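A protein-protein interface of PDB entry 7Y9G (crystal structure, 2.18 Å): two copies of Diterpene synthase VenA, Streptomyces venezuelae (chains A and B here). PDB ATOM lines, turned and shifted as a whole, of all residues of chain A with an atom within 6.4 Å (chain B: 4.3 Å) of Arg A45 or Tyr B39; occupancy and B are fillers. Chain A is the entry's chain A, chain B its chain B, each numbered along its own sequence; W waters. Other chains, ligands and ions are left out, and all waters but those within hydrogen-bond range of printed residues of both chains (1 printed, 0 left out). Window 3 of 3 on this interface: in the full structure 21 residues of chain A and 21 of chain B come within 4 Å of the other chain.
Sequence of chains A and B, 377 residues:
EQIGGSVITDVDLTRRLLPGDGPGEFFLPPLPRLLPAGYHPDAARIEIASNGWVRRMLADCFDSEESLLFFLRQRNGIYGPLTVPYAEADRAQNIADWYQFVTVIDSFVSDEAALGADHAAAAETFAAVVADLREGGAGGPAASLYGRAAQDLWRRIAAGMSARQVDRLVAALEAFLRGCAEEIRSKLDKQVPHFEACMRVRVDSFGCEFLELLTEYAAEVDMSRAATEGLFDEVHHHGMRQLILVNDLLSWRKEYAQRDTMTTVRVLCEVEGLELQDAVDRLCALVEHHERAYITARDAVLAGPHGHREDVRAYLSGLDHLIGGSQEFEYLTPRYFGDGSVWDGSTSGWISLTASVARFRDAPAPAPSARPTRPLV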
ATOM      1  N   PRO A  41      20.595  -6.075 -13.814  1.00  0.00           N
ATOM      2  CA  PRO A  41      20.939  -6.879 -12.640  1.00  0.00           C
ATOM      3  C   PRO A  41      20.410  -6.296 -11.321  1.00  0.00           C
ATOM      4  O   PRO A  41      20.322  -7.032 -10.394  1.00  0.00           O
ATOM      5  CB  PRO A  41      22.473  -6.941 -12.678  1.00  0.00           C
ATOM      6  CG  PRO A  41      22.897  -5.803 -13.576  1.00  0.00           C
ATOM      7  CD  PRO A  41      21.776  -5.648 -14.582  1.00  0.00           C
ATOM      8  N   ASP A  42      19.979  -5.027 -11.300  1.00  0.00           N
ATOM      9  CA  ASP A  42      19.362  -4.360 -10.125  1.00  0.00           C
ATOM     10  C   ASP A  42      17.863  -4.082 -10.344  1.00  0.00           C
ATOM     11  O   ASP A  42      17.350  -3.156  -9.691  1.00  0.00           O
ATOM     12  CB  ASP A  42      20.096  -3.047  -9.843  1.00  0.00           C
ATOM     13  CG  ASP A  42      21.566  -3.234  -9.537  1.00  0.00           C
ATOM     14  OD1 ASP A  42      21.866  -4.129  -8.737  1.00  0.00           O
ATOM     15  OD2 ASP A  42      22.402  -2.480 -10.113  1.00  0.00           O
ATOM     16  N   ALA A  43      17.185  -4.780 -11.257  1.00  0.00           N
ATOM     17  CA  ALA A  43      15.805  -4.423 -11.697  1.00  0.00           C
ATOM     18  C   ALA A  43      14.844  -4.371 -10.502  1.00  0.00           C
ATOM     19  O   ALA A  43      14.173  -3.355 -10.369  1.00  0.00           O
ATOM     20  CB  ALA A  43      15.281  -5.389 -12.718  1.00  0.00           C
ATOM     21  N   ALA A  44      14.775  -5.419  -9.664  1.00  0.00           N
ATOM     22  CA  ALA A  44      13.831  -5.492  -8.518  1.00  0.00           C
ATOM     23  C   ALA A  44      14.034  -4.289  -7.575  1.00  0.00           C
ATOM     24  O   ALA A  44      13.019  -3.642  -7.187  1.00  0.00           O
ATOM     25  CB  ALA A  44      13.969  -6.804  -7.784  1.00  0.00           C
ATOM     26  N   ARG A  45      15.287  -3.980  -7.230  1.00  0.00           N
ATOM     27  CA  ARG A  45      15.631  -2.888  -6.280  1.00  0.00           C
ATOM     28  C   ARG A  45      15.287  -1.551  -6.933  1.00  0.00           C
ATOM     29  O   ARG A  45      14.719  -0.701  -6.263  1.00  0.00           O
ATOM     30  CB  ARG A  45      17.111  -2.939  -5.889  1.00  0.00           C
ATOM     31  CG  ARG A  45      17.491  -1.938  -4.811  1.00  0.00           C
ATOM     32  CD  ARG A  45      18.880  -2.171  -4.240  1.00  0.00           C
ATOM     33  NE  ARG A  45      19.923  -2.114  -5.253  1.00  0.00           N
ATOM     34  CZ  ARG A  45      20.297  -1.021  -5.931  1.00  0.00           C
ATOM     35  NH1 ARG A  45      19.691   0.145  -5.750  1.00  0.00           N
ATOM     36  NH2 ARG A  45      21.275  -1.102  -6.819  1.00  0.00           N
ATOM     37  N   ILE A  46      15.623  -1.378  -8.204  1.00  0.00           N
ATOM     38  CA  ILE A  46      15.309  -0.134  -8.965  1.00  0.00           C
ATOM     39  C   ILE A  46      13.795   0.094  -8.960  1.00  0.00           C
ATOM     40  O   ILE A  46      13.365   1.287  -8.797  1.00  0.00           O
ATOM     41  CB  ILE A  46      15.894  -0.203 -10.387  1.00  0.00           C
ATOM     42  CG1 ILE A  46      17.416  -0.019 -10.347  1.00  0.00           C
ATOM     43  CG2 ILE A  46      15.220   0.810 -11.315  1.00  0.00           C
ATOM     44  CD1 ILE A  46      18.120  -0.153 -11.704  1.00  0.00           C
ATOM     45  N   GLU A  47      13.009  -0.966  -9.132  1.00  0.00           N
ATOM     46  CA  GLU A  47      11.523  -0.877  -9.174  1.00  0.00           C
ATOM     47  C   GLU A  47      11.037  -0.261  -7.852  1.00  0.00           C
ATOM     48  O   GLU A  47      10.200   0.698  -7.889  1.00  0.00           O
ATOM     49  CB  GLU A  47      10.901  -2.264  -9.405  1.00  0.00           C
ATOM     50  CG  GLU A  47       9.380  -2.269  -9.263  1.00  0.00           C
ATOM     51  CD  GLU A  47       8.716  -3.625  -9.405  1.00  0.00           C
ATOM     52  OE1 GLU A  47       9.461  -4.616  -9.497  1.00  0.00           O
ATOM     53  OE2 GLU A  47       7.442  -3.711  -9.354  1.00  0.00           O
ATOM     54  N   ILE A  48      11.560  -0.791  -6.740  1.00  0.00           N
ATOM     55  CA  ILE A  48      11.221  -0.343  -5.358  1.00  0.00           C
ATOM     56  C   ILE A  48      11.634   1.121  -5.187  1.00  0.00           C
ATOM     57  O   ILE A  48      10.812   1.906  -4.667  1.00  0.00           O
ATOM     58  CB  ILE A  48      11.852  -1.252  -4.278  1.00  0.00           C
ATOM     59  CG1 ILE A  48      11.401  -2.707  -4.383  1.00  0.00           C
ATOM     60  CG2 ILE A  48      11.571  -0.689  -2.884  1.00  0.00           C
ATOM     61  CD1 ILE A  48       9.896  -2.869  -4.579  1.00  0.00           C
ATOM     62  N   ALA A  49      12.867   1.482  -5.565  1.00  0.00           N
ATOM     63  CA  ALA A  49      13.371   2.866  -5.394  1.00  0.00           C
ATOM     64  C   ALA A  49      12.530   3.793  -6.280  1.00  0.00           C
ATOM     65  O   ALA A  49      12.300   4.950  -5.915  1.00  0.00           O
ATOM     66  CB  ALA A  49      14.842   2.948  -5.731  1.00  0.00           C
ATOM     67  N   SER A  50      12.069   3.297  -7.422  1.00  0.00           N
ATOM     68  CA  SER A  50      11.186   4.065  -8.324  1.00  0.00           C
ATOM     69  C   SER A  50       9.841   4.295  -7.608  1.00  0.00           C
ATOM     70  O   SER A  50       9.371   5.453  -7.611  1.00  0.00           O
ATOM     71  CB  SER A  50      11.055   3.394  -9.650  1.00  0.00           C
ATOM     72  OG  SER A  50      10.434   4.262 -10.557  1.00  0.00           O
ATOM     73  N   ALA A  89      23.466   1.803 -13.131  1.00  0.00           N
ATOM     74  CA  ALA A  89      22.370   1.823 -12.138  1.00  0.00           C
ATOM     75  C   ALA A  89      21.698   3.204 -12.093  1.00  0.00           C
ATOM     76  O   ALA A  89      20.466   3.254 -12.125  1.00  0.00           O
ATOM     77  CB  ALA A  89      22.923   1.414 -10.793  1.00  0.00           C
ATOM     78  N   GLN A  93      17.895   3.966 -13.117  1.00  0.00           N
ATOM     79  CA  GLN A  93      16.985   4.490 -12.072  1.00  0.00           C
ATOM     80  C   GLN A  93      16.278   5.723 -12.617  1.00  0.00           C
ATOM     81  O   GLN A  93      15.082   5.860 -12.388  1.00  0.00           O
ATOM     82  CB  GLN A  93      17.708   4.860 -10.774  1.00  0.00           C
ATOM     83  CG  GLN A  93      16.732   5.202  -9.642  1.00  0.00           C
ATOM     84  CD  GLN A  93      15.878   4.022  -9.222  1.00  0.00           C
ATOM     85  OE1 GLN A  93      16.379   3.043  -8.701  1.00  0.00           O
ATOM     86  NE2 GLN A  93      14.574   4.082  -9.460  1.00  0.00           N
ATOM     87  N   GLY B  38      21.903  -8.443  -0.697  1.00  0.00           N
ATOM     88  CA  GLY B  38      21.994  -8.336  -2.164  1.00  0.00           C
ATOM     89  C   GLY B  38      20.897  -9.109  -2.858  1.00  0.00           C
ATOM     90  O   GLY B  38      20.458 -10.159  -2.328  1.00  0.00           O
ATOM     91  N   TYR B  39      20.472  -8.600  -4.013  1.00  0.00           N
ATOM     92  CA  TYR B  39      19.494  -9.233  -4.932  1.00  0.00           C
ATOM     93  C   TYR B  39      20.284 -10.059  -5.950  1.00  0.00           C
ATOM     94  O   TYR B  39      21.224  -9.517  -6.513  1.00  0.00           O
ATOM     95  CB  TYR B  39      18.663  -8.153  -5.641  1.00  0.00           C
ATOM     96  CG  TYR B  39      17.667  -7.399  -4.791  1.00  0.00           C
ATOM     97  CD1 TYR B  39      18.066  -6.354  -3.979  1.00  0.00           C
ATOM     98  CD2 TYR B  39      16.313  -7.692  -4.835  1.00  0.00           C
ATOM     99  CE1 TYR B  39      17.155  -5.649  -3.204  1.00  0.00           C
ATOM    100  CE2 TYR B  39      15.391  -6.995  -4.071  1.00  0.00           C
ATOM    101  CZ  TYR B  39      15.811  -5.953  -3.266  1.00  0.00           C
ATOM    102  OH  TYR B  39      14.920  -5.253  -2.507  1.00  0.00           O
ATOM    103  N   HIS B  40      19.931 -11.320  -6.185  1.00  0.00           N
ATOM    104  CA  HIS B  40      20.449 -12.078  -7.349  1.00  0.00           C
ATOM    105  C   HIS B  40      20.304 -11.207  -8.594  1.00  0.00           C
ATOM    106  O   HIS B  40      19.337 -10.457  -8.742  1.00  0.00           O
ATOM    107  CB  HIS B  40      19.726 -13.416  -7.498  1.00  0.00           C
ATOM    108  CG  HIS B  40      20.408 -14.353  -8.434  1.00  0.00           C
ATOM    109  ND1 HIS B  40      20.238 -14.280  -9.803  1.00  0.00           N
ATOM    110  CD2 HIS B  40      21.265 -15.373  -8.209  1.00  0.00           C
ATOM    111  CE1 HIS B  40      20.978 -15.209 -10.373  1.00  0.00           C
ATOM    112  NE2 HIS B  40      21.612 -15.891  -9.426  1.00  0.00           N
ATOM    113  N   PRO B  41      21.281 -11.226  -9.518  1.00  0.00           N
ATOM    114  CA  PRO B  41      21.142 -10.472 -10.760  1.00  0.00           C
ATOM    115  C   PRO B  41      19.896 -10.868 -11.566  1.00  0.00           C
ATOM    116  O   PRO B  41      19.487 -10.083 -12.362  1.00  0.00           O
ATOM    117  CB  PRO B  41      22.410 -10.814 -11.574  1.00  0.00           C
ATOM    118  CG  PRO B  41      23.384 -11.420 -10.568  1.00  0.00           C
ATOM    119  CD  PRO B  41      22.548 -11.966  -9.429  1.00  0.00           C
ATOM    120  N   PRO B  81      16.059 -15.568  -4.187  1.00  0.00           N
ATOM    121  CA  PRO B  81      17.144 -14.810  -4.796  1.00  0.00           C
ATOM    122  C   PRO B  81      17.704 -13.665  -3.946  1.00  0.00           C
ATOM    123  O   PRO B  81      18.815 -13.211  -4.227  1.00  0.00           O
ATOM    124  CB  PRO B  81      16.573 -14.255  -6.104  1.00  0.00           C
ATOM    125  CG  PRO B  81      15.122 -14.620  -6.129  1.00  0.00           C
ATOM    126  CD  PRO B  81      14.832 -15.563  -4.985  1.00  0.00           C
ATOM    127  N   LEU B  82      16.959 -13.226  -2.930  1.00  0.00           N
ATOM    128  CA  LEU B  82      17.455 -12.233  -1.945  1.00  0.00           C
ATOM    129  C   LEU B  82      18.322 -12.937  -0.902  1.00  0.00           C
ATOM    130  O   LEU B  82      19.150 -12.206  -0.294  1.00  0.00           O
ATOM    131  CB  LEU B  82      16.302 -11.470  -1.281  1.00  0.00           C
ATOM    132  CG  LEU B  82      16.013 -10.094  -1.879  1.00  0.00           C
ATOM    133  CD1 LEU B  82      14.647  -9.593  -1.452  1.00  0.00           C
ATOM    134  CD2 LEU B  82      17.076  -9.093  -1.504  1.00  0.00           C
ATOM    135  N   PRO B  85      22.224 -14.170  -3.479  1.00  0.00           N
ATOM    136  CA  PRO B  85      22.430 -13.303  -4.633  1.00  0.00           C
ATOM    137  C   PRO B  85      23.669 -13.716  -5.457  1.00  0.00           C
ATOM    138  O   PRO B  85      23.833 -13.264  -6.571  1.00  0.00           O
ATOM    139  CB  PRO B  85      22.605 -11.923  -3.982  1.00  0.00           C
ATOM    140  CG  PRO B  85      23.194 -12.244  -2.633  1.00  0.00           C
ATOM    141  CD  PRO B  85      22.440 -13.480  -2.198  1.00  0.00           C
ATOM    142  N   GLU B 328      15.707  -7.717   4.047  1.00  0.00           N
ATOM    143  CA  GLU B 328      15.315  -6.868   2.889  1.00  0.00           C
ATOM    144  C   GLU B 328      13.959  -7.401   2.380  1.00  0.00           C
ATOM    145  O   GLU B 328      13.034  -6.602   2.216  1.00  0.00           O
ATOM    146  CB  GLU B 328      16.440  -6.860   1.853  1.00  0.00           C
ATOM    147  CG  GLU B 328      16.074  -6.191   0.550  1.00  0.00           C
ATOM    148  CD  GLU B 328      16.214  -4.686   0.540  1.00  0.00           C
ATOM    149  OE1 GLU B 328      16.534  -4.096   1.584  1.00  0.00           O
ATOM    150  OE2 GLU B 328      16.006  -4.113  -0.521  1.00  0.00           O
ATOM    151  N   LEU B 332       9.756  -5.991   2.149  1.00  0.00           N
ATOM    152  CA  LEU B 332       9.237  -5.866   0.760  1.00  0.00           C
ATOM    153  C   LEU B 332       7.821  -6.481   0.689  1.00  0.00           C
ATOM    154  O   LEU B 332       6.958  -5.946  -0.049  1.00  0.00           O
ATOM    155  CB  LEU B 332      10.261  -6.509  -0.191  1.00  0.00           C
ATOM    156  CG  LEU B 332       9.957  -6.486  -1.692  1.00  0.00           C
ATOM    157  CD1 LEU B 332      11.222  -6.731  -2.509  1.00  0.00           C
ATOM    158  CD2 LEU B 332       8.909  -7.520  -2.061  1.00  0.00           C
ATOM    159  N   TRP B 343       5.901  -1.918  -1.657  1.00  0.00           N
ATOM    160  CA  TRP B 343       7.048  -1.351  -0.906  1.00  0.00           C
ATOM    161  C   TRP B 343       7.619  -0.130  -1.636  1.00  0.00           C
ATOM    162  O   TRP B 343       7.869  -0.203  -2.877  1.00  0.00           O
ATOM    163  CB  TRP B 343       8.106  -2.418  -0.673  1.00  0.00           C
ATOM    164  CG  TRP B 343       9.140  -2.017   0.323  1.00  0.00           C
ATOM    165  CD1 TRP B 343       8.975  -1.229   1.431  1.00  0.00           C
ATOM    166  CD2 TRP B 343      10.515  -2.419   0.302  1.00  0.00           C
ATOM    167  NE1 TRP B 343      10.170  -1.099   2.085  1.00  0.00           N
ATOM    168  CE2 TRP B 343      11.132  -1.814   1.414  1.00  0.00           C
ATOM    169  CE3 TRP B 343      11.276  -3.243  -0.533  1.00  0.00           C
ATOM    170  CZ2 TRP B 343      12.480  -2.020   1.705  1.00  0.00           C
ATOM    171  CZ3 TRP B 343      12.611  -3.423  -0.252  1.00  0.00           C
ATOM    172  CH2 TRP B 343      13.208  -2.809   0.847  1.00  0.00           C
HETATM  173  O   HOH W   1      18.395  -8.007  -9.074  1.00  0.00           O
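Water W1 bridges O of Pro A41 (2.5 Å) and O of His B40 (2.6 Å).
Arg A45 touches just one residue of chain B: Tyr B39 (3.8 Å). Of the printed residues of chain B, Ile A48 touches Trp B343. Ala A89 touches none of the printed residues of chain B. Tyr B39 touches two residues of chain A. Of the printed residues of chain A, Trp B343 touches Ile A48 (3.5 Å).
His B40 touches Pro A41. CA of Pro A41 touches O of Pro B41, 3.5 Å away. Tyr B39 touches Ala A44 (CD2 to CB, 3.9 Å). CB of Arg A45 touches CE1 of Tyr B39, at 3.8 Å. Ile A48 touches Trp B343.
The side-chain hydroxyl (OH) of Tyr B39 is in hydrogen-bond range of the side-chain carboxylate (OE2) of Glu B328 (2.5 Å). The backbone carbonyl oxygen (O) of Pro B81 lies within hydrogen-bond range of the backbone NH (N) of His B40 (2.9 Å). The guanidinium group (NH2) of Arg A45 lies within salt-bridge range of the side-chain carboxylate (OD1) of Asp A42 (3.6 Å).
Of the 12 printed residues of chain A, 4 touch a printed residue of chain B. Printed residues of chain A that touch a printed residue of chain B: Pro A41, Ala A44, Arg A45 and Ile A48. Hydrophobic or aromatic side chains of chain A that line the printed part of chain B: Ala A44 and Ile A48. Among the printed residues, 5 pairs touch across the chains. Among the printed residues, no Asp or Glu carboxylate lies within 4 Å of a Lys or Arg side-chain nitrogen of the other chain.
Pro B41 touches its own counterpart, Pro A41. Of the 5 pairs that touch across the chains among the printed residues, 1 has its exchanged pair printed and touching as well.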
